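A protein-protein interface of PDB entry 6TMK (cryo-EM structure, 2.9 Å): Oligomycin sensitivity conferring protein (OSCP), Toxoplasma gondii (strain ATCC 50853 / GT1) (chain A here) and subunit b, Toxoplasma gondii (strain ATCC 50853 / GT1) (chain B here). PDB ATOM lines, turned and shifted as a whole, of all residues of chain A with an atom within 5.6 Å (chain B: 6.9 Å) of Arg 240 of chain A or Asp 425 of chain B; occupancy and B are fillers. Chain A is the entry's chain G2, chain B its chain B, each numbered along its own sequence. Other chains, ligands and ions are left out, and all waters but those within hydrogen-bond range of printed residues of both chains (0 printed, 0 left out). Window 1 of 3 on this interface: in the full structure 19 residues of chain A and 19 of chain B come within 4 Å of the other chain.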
ATOM      1  N   ASP A 234      20.415 -28.866   0.065  1.00  0.00           N
ATOM      2  CA  ASP A 234      19.442 -29.850  -0.407  1.00  0.00           C
ATOM      3  C   ASP A 234      18.695 -29.314  -1.628  1.00  0.00           C
ATOM      4  O   ASP A 234      17.478 -29.132  -1.628  1.00  0.00           O
ATOM      5  CB  ASP A 234      18.475 -30.215   0.714  1.00  0.00           C
ATOM      6  CG  ASP A 234      17.739 -31.514   0.448  1.00  0.00           C
ATOM      7  OD1 ASP A 234      17.650 -31.918  -0.731  1.00  0.00           O
ATOM      8  OD2 ASP A 234      17.246 -32.129   1.416  1.00  0.00           O
ATOM      9  N   SER A 236      16.932 -30.106  -4.303  1.00  0.00           N
ATOM     10  CA  SER A 236      16.177 -31.242  -4.806  1.00  0.00           C
ATOM     11  C   SER A 236      14.775 -30.783  -5.185  1.00  0.00           C
ATOM     12  O   SER A 236      14.355 -29.664  -4.877  1.00  0.00           O
ATOM     13  CB  SER A 236      16.108 -32.373  -3.771  1.00  0.00           C
ATOM     14  OG  SER A 236      15.062 -33.280  -4.071  1.00  0.00           O
ATOM     15  N   VAL A 237      14.052 -31.673  -5.863  1.00  0.00           N
ATOM     16  CA  VAL A 237      12.679 -31.386  -6.266  1.00  0.00           C
ATOM     17  C   VAL A 237      11.714 -31.714  -5.134  1.00  0.00           C
ATOM     18  O   VAL A 237      11.001 -30.838  -4.629  1.00  0.00           O
ATOM     19  CB  VAL A 237      12.319 -32.158  -7.548  1.00  0.00           C
ATOM     20  CG1 VAL A 237      10.841 -31.989  -7.877  1.00  0.00           C
ATOM     21  CG2 VAL A 237      13.183 -31.702  -8.707  1.00  0.00           C
ATOM     22  N   ALA A 238      11.668 -32.990  -4.739  1.00  0.00           N
ATOM     23  CA  ALA A 238      10.675 -33.449  -3.775  1.00  0.00           C
ATOM     24  C   ALA A 238      10.835 -32.755  -2.431  1.00  0.00           C
ATOM     25  O   ALA A 238       9.841 -32.501  -1.744  1.00  0.00           O
ATOM     26  CB  ALA A 238      10.779 -34.964  -3.595  1.00  0.00           C
ATOM     27  N   THR A 239      12.066 -32.411  -2.054  1.00  0.00           N
ATOM     28  CA  THR A 239      12.293 -31.816  -0.741  1.00  0.00           C
ATOM     29  C   THR A 239      11.754 -30.392  -0.695  1.00  0.00           C
ATOM     30  O   THR A 239      11.014 -30.028   0.227  1.00  0.00           O
ATOM     31  CB  THR A 239      13.786 -31.834  -0.404  1.00  0.00           C
ATOM     32  OG1 THR A 239      14.473 -30.861  -1.201  1.00  0.00           O
ATOM     33  CG2 THR A 239      14.383 -33.213  -0.658  1.00  0.00           C
ATOM     34  N   ARG A 240      12.120 -29.569  -1.680  1.00  0.00           N
ATOM     35  CA  ARG A 240      11.543 -28.233  -1.775  1.00  0.00           C
ATOM     36  C   ARG A 240      10.026 -28.301  -1.899  1.00  0.00           C
ATOM     37  O   ARG A 240       9.312 -27.505  -1.283  1.00  0.00           O
ATOM     38  CB  ARG A 240      12.139 -27.473  -2.956  1.00  0.00           C
ATOM     39  CG  ARG A 240      11.489 -26.113  -3.168  1.00  0.00           C
ATOM     40  CD  ARG A 240      12.408 -25.131  -3.874  1.00  0.00           C
ATOM     41  NE  ARG A 240      12.205 -23.763  -3.397  1.00  0.00           N
ATOM     42  CZ  ARG A 240      11.453 -22.848  -4.004  1.00  0.00           C
ATOM     43  NH1 ARG A 240      11.349 -21.633  -3.486  1.00  0.00           N
ATOM     44  NH2 ARG A 240      10.790 -23.141  -5.114  1.00  0.00           N
ATOM     45  N   LEU A 241       9.515 -29.254  -2.684  1.00  0.00           N
ATOM     46  CA  LEU A 241       8.071 -29.393  -2.850  1.00  0.00           C
ATOM     47  C   LEU A 241       7.390 -29.651  -1.511  1.00  0.00           C
ATOM     48  O   LEU A 241       6.416 -28.975  -1.155  1.00  0.00           O
ATOM     49  CB  LEU A 241       7.769 -30.516  -3.843  1.00  0.00           C
ATOM     50  CG  LEU A 241       6.294 -30.786  -4.153  1.00  0.00           C
ATOM     51  CD1 LEU A 241       6.127 -31.175  -5.613  1.00  0.00           C
ATOM     52  CD2 LEU A 241       5.729 -31.871  -3.246  1.00  0.00           C
ATOM     53  N   ASP A 242       7.872 -30.643  -0.762  1.00  0.00           N
ATOM     54  CA  ASP A 242       7.226 -31.003   0.495  1.00  0.00           C
ATOM     55  C   ASP A 242       7.381 -29.891   1.524  1.00  0.00           C
ATOM     56  O   ASP A 242       6.448 -29.615   2.289  1.00  0.00           O
ATOM     57  CB  ASP A 242       7.806 -32.312   1.028  1.00  0.00           C
ATOM     58  CG  ASP A 242       7.467 -32.549   2.487  1.00  0.00           C
ATOM     59  OD1 ASP A 242       6.408 -33.150   2.762  1.00  0.00           O
ATOM     60  OD2 ASP A 242       8.259 -32.129   3.358  1.00  0.00           O
ATOM     61  N   ARG A 243       8.554 -29.255   1.579  1.00  0.00           N
ATOM     62  CA  ARG A 243       8.731 -28.127   2.486  1.00  0.00           C
ATOM     63  C   ARG A 243       7.743 -27.014   2.156  1.00  0.00           C
ATOM     64  O   ARG A 243       7.121 -26.436   3.055  1.00  0.00           O
ATOM     65  CB  ARG A 243      10.167 -27.614   2.400  1.00  0.00           C
ATOM     66  CG  ARG A 243      10.635 -26.848   3.623  1.00  0.00           C
ATOM     67  CD  ARG A 243      12.147 -26.905   3.744  1.00  0.00           C
ATOM     68  NE  ARG A 243      12.799 -26.711   2.449  1.00  0.00           N
ATOM     69  CZ  ARG A 243      13.420 -27.663   1.755  1.00  0.00           C
ATOM     70  NH1 ARG A 243      13.980 -27.367   0.590  1.00  0.00           N
ATOM     71  NH2 ARG A 243      13.481 -28.910   2.205  1.00  0.00           N
ATOM     72  N   LEU A 244       7.567 -26.720   0.867  1.00  0.00           N
ATOM     73  CA  LEU A 244       6.626 -25.685   0.458  1.00  0.00           C
ATOM     74  C   LEU A 244       5.212 -26.058   0.874  1.00  0.00           C
ATOM     75  O   LEU A 244       4.451 -25.216   1.362  1.00  0.00           O
ATOM     76  CB  LEU A 244       6.717 -25.477  -1.056  1.00  0.00           C
ATOM     77  CG  LEU A 244       6.076 -24.214  -1.628  1.00  0.00           C
ATOM     78  CD1 LEU A 244       6.837 -22.972  -1.195  1.00  0.00           C
ATOM     79  CD2 LEU A 244       6.019 -24.302  -3.145  1.00  0.00           C
ATOM     80  N   GLN A 245       4.816 -27.306   0.614  1.00  0.00           N
ATOM     81  CA  GLN A 245       3.481 -27.762   0.987  1.00  0.00           C
ATOM     82  C   GLN A 245       3.249 -27.599   2.487  1.00  0.00           C
ATOM     83  O   GLN A 245       2.228 -27.046   2.917  1.00  0.00           O
ATOM     84  CB  GLN A 245       3.297 -29.221   0.566  1.00  0.00           C
ATOM     85  CG  GLN A 245       2.268 -29.987   1.381  1.00  0.00           C
ATOM     86  CD  GLN A 245       1.898 -31.314   0.748  1.00  0.00           C
ATOM     87  OE1 GLN A 245       2.407 -31.672  -0.313  1.00  0.00           O
ATOM     88  NE2 GLN A 245       1.009 -32.053   1.399  1.00  0.00           N
ATOM     89  N   PHE B 395       1.310 -31.000  -9.944  1.00  0.00           N
ATOM     90  CA  PHE B 395       2.730 -30.882 -10.259  1.00  0.00           C
ATOM     91  C   PHE B 395       3.393 -32.250 -10.337  1.00  0.00           C
ATOM     92  O   PHE B 395       4.255 -32.480 -11.193  1.00  0.00           O
ATOM     93  CB  PHE B 395       3.450 -30.011  -9.234  1.00  0.00           C
ATOM     94  CG  PHE B 395       4.813 -29.578  -9.683  1.00  0.00           C
ATOM     95  CD1 PHE B 395       4.961 -28.615 -10.665  1.00  0.00           C
ATOM     96  CD2 PHE B 395       5.949 -30.157  -9.143  1.00  0.00           C
ATOM     97  CE1 PHE B 395       6.215 -28.225 -11.089  1.00  0.00           C
ATOM     98  CE2 PHE B 395       7.205 -29.773  -9.563  1.00  0.00           C
ATOM     99  CZ  PHE B 395       7.338 -28.807 -10.541  1.00  0.00           C
ATOM    100  N   ALA B 408      15.044 -28.116 -16.807  1.00  0.00           N
ATOM    101  CA  ALA B 408      14.783 -26.830 -16.170  1.00  0.00           C
ATOM    102  C   ALA B 408      15.172 -26.856 -14.696  1.00  0.00           C
ATOM    103  O   ALA B 408      15.796 -25.914 -14.196  1.00  0.00           O
ATOM    104  CB  ALA B 408      13.310 -26.457 -16.330  1.00  0.00           C
ATOM    105  N   ALA B 409      14.837 -27.938 -13.988  1.00  0.00           N
ATOM    106  CA  ALA B 409      15.222 -28.055 -12.586  1.00  0.00           C
ATOM    107  C   ALA B 409      16.731 -28.201 -12.443  1.00  0.00           C
ATOM    108  O   ALA B 409      17.327 -27.680 -11.492  1.00  0.00           O
ATOM    109  CB  ALA B 409      14.506 -29.243 -11.943  1.00  0.00           C
ATOM    110  N   SER B 412      18.058 -24.881 -12.761  1.00  0.00           N
ATOM    111  CA  SER B 412      17.674 -24.099 -11.593  1.00  0.00           C
ATOM    112  C   SER B 412      18.637 -24.364 -10.448  1.00  0.00           C
ATOM    113  O   SER B 412      19.126 -23.432  -9.802  1.00  0.00           O
ATOM    114  CB  SER B 412      16.239 -24.431 -11.185  1.00  0.00           C
ATOM    115  OG  SER B 412      16.196 -25.596 -10.381  1.00  0.00           O
ATOM    116  N   ALA B 413      18.921 -25.640 -10.181  1.00  0.00           N
ATOM    117  CA  ALA B 413      19.882 -25.982  -9.138  1.00  0.00           C
ATOM    118  C   ALA B 413      21.252 -25.398  -9.459  1.00  0.00           C
ATOM    119  O   ALA B 413      21.938 -24.863  -8.576  1.00  0.00           O
ATOM    120  CB  ALA B 413      19.979 -27.499  -8.985  1.00  0.00           C
ATOM    121  N   MET B 424      13.383 -18.701 -11.640  1.00  0.00           N
ATOM    122  CA  MET B 424      12.958 -19.497 -10.496  1.00  0.00           C
ATOM    123  C   MET B 424      12.734 -20.951 -10.896  1.00  0.00           C
ATOM    124  O   MET B 424      12.498 -21.255 -12.065  1.00  0.00           O
ATOM    125  CB  MET B 424      11.677 -18.920  -9.889  1.00  0.00           C
ATOM    126  CG  MET B 424      11.258 -19.580  -8.585  1.00  0.00           C
ATOM    127  SD  MET B 424      10.077 -18.588  -7.653  1.00  0.00           S
ATOM    128  CE  MET B 424      10.512 -19.036  -5.975  1.00  0.00           C
ATOM    129  N   ASP B 425      12.811 -21.847  -9.911  1.00  0.00           N
ATOM    130  CA  ASP B 425      12.632 -23.262 -10.174  1.00  0.00           C
ATOM    131  C   ASP B 425      11.230 -23.517 -10.724  1.00  0.00           C
ATOM    132  O   ASP B 425      10.300 -22.736 -10.483  1.00  0.00           O
ATOM    133  CB  ASP B 425      12.856 -24.070  -8.898  1.00  0.00           C
ATOM    134  CG  ASP B 425      11.832 -23.764  -7.829  1.00  0.00           C
ATOM    135  OD1 ASP B 425      11.533 -22.570  -7.614  1.00  0.00           O
ATOM    136  OD2 ASP B 425      11.328 -24.716  -7.199  1.00  0.00           O
ATOM    137  N   PRO B 426      11.037 -24.635 -11.432  1.00  0.00           N
ATOM    138  CA  PRO B 426       9.707 -24.904 -11.988  1.00  0.00           C
ATOM    139  C   PRO B 426       8.688 -25.273 -10.934  1.00  0.00           C
ATOM    140  O   PRO B 426       7.489 -25.120 -11.185  1.00  0.00           O
ATOM    141  CB  PRO B 426       9.967 -26.063 -12.956  1.00  0.00           C
ATOM    142  CG  PRO B 426      11.087 -26.805 -12.312  1.00  0.00           C
ATOM    143  CD  PRO B 426      11.978 -25.730 -11.728  1.00  0.00           C
ATOM    144  N   VAL B 427       9.116 -25.653  -9.730  1.00  0.00           N
ATOM    145  CA  VAL B 427       8.161 -26.015  -8.689  1.00  0.00           C
ATOM    146  C   VAL B 427       7.462 -24.760  -8.188  1.00  0.00           C
ATOM    147  O   VAL B 427       6.228 -24.649  -8.222  1.00  0.00           O
ATOM    148  CB  VAL B 427       8.865 -26.761  -7.541  1.00  0.00           C
ATOM    149  CG1 VAL B 427       7.842 -27.392  -6.610  1.00  0.00           C
ATOM    150  CG2 VAL B 427       9.828 -27.811  -8.085  1.00  0.00           C
ATOM    151  N   GLY B 428       8.252 -23.798  -7.708  1.00  0.00           N
ATOM    152  CA  GLY B 428       7.698 -22.510  -7.334  1.00  0.00           C
ATOM    153  C   GLY B 428       6.995 -21.831  -8.491  1.00  0.00           C
ATOM    154  O   GLY B 428       5.965 -21.178  -8.306  1.00  0.00           O
ATOM    155  N   ALA B 429       7.526 -21.991  -9.708  1.00  0.00           N
ATOM    156  CA  ALA B 429       6.892 -21.364 -10.862  1.00  0.00           C
ATOM    157  C   ALA B 429       5.484 -21.906 -11.066  1.00  0.00           C
ATOM    158  O   ALA B 429       4.524 -21.138 -11.204  1.00  0.00           O
ATOM    159  CB  ALA B 429       7.744 -21.586 -12.112  1.00  0.00           C
ATOM    160  N   HIS B 430       5.334 -23.232 -11.063  1.00  0.00           N
ATOM    161  CA  HIS B 430       4.025 -23.827 -11.302  1.00  0.00           C
ATOM    162  C   HIS B 430       3.078 -23.522 -10.151  1.00  0.00           C
ATOM    163  O   HIS B 430       1.887 -23.272 -10.370  1.00  0.00           O
ATOM    164  CB  HIS B 430       4.155 -25.335 -11.501  1.00  0.00           C
ATOM    165  CG  HIS B 430       2.876 -26.081 -11.279  1.00  0.00           C
ATOM    166  ND1 HIS B 430       2.524 -26.609 -10.056  1.00  0.00           N
ATOM    167  CD2 HIS B 430       1.865 -26.388 -12.126  1.00  0.00           C
ATOM    168  CE1 HIS B 430       1.351 -27.208 -10.158  1.00  0.00           C
ATOM    169  NE2 HIS B 430       0.929 -27.088 -11.404  1.00  0.00           N
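OD2 of Asp 425 of chain B is in salt-bridge range of NH2 of Arg 240 of chain A, at 2.7 Å.
OD2 of Asp 425 of chain B lies close to N of Val 427 of chain B (3.5 Å). The side-chain carboxylate (OD2) of Asp 425 of chain B sits at hydrogen-bond distance from the backbone NH (N) of Gly 428 of chain B (3.3 Å).
Arg 240 of chain A touches Met 424 of chain B (NH1 to CE, 3.7 Å). Gly 428 of chain B touches Arg 240 of chain A. Leu 241 of chain A touches Phe 395 of chain B (CD1 to CD2, 3.7 Å).
Of the printed residues of chain B, Arg 240 of chain A touches Met 424, Asp 425 and Gly 428. Printed residues of chain B within 4 Å of Leu 241 of chain A: Phe 395 (3.7 Å). Arg 243 of chain A touches none of the printed residues of chain B. Of the printed residues of chain A, Met 424 of chain B touches Arg 240 (3.7 Å). Asp 425 of chain B touches just one residue of chain A: Arg 240 (2.7 Å). Of the printed residues of chain A, Gly 428 of chain B touches Arg 240 (3.7 Å).
Of the 11 printed residues of chain A, 2 touch a printed residue of chain B. Hydrophobic or aromatic side chains of chain A that line the printed part of chain B: Leu 241. Along chain A the printed residues that touch a printed residue of chain B span positions 240 to 241. Among the printed residues, 4 pairs touch across the chains. Among the printed residues, Asp or Glu carboxylates within 4 Å of a Lys or Arg side-chain nitrogen of the other chain: Arg 240 of chain A with Asp 425 of chain B.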
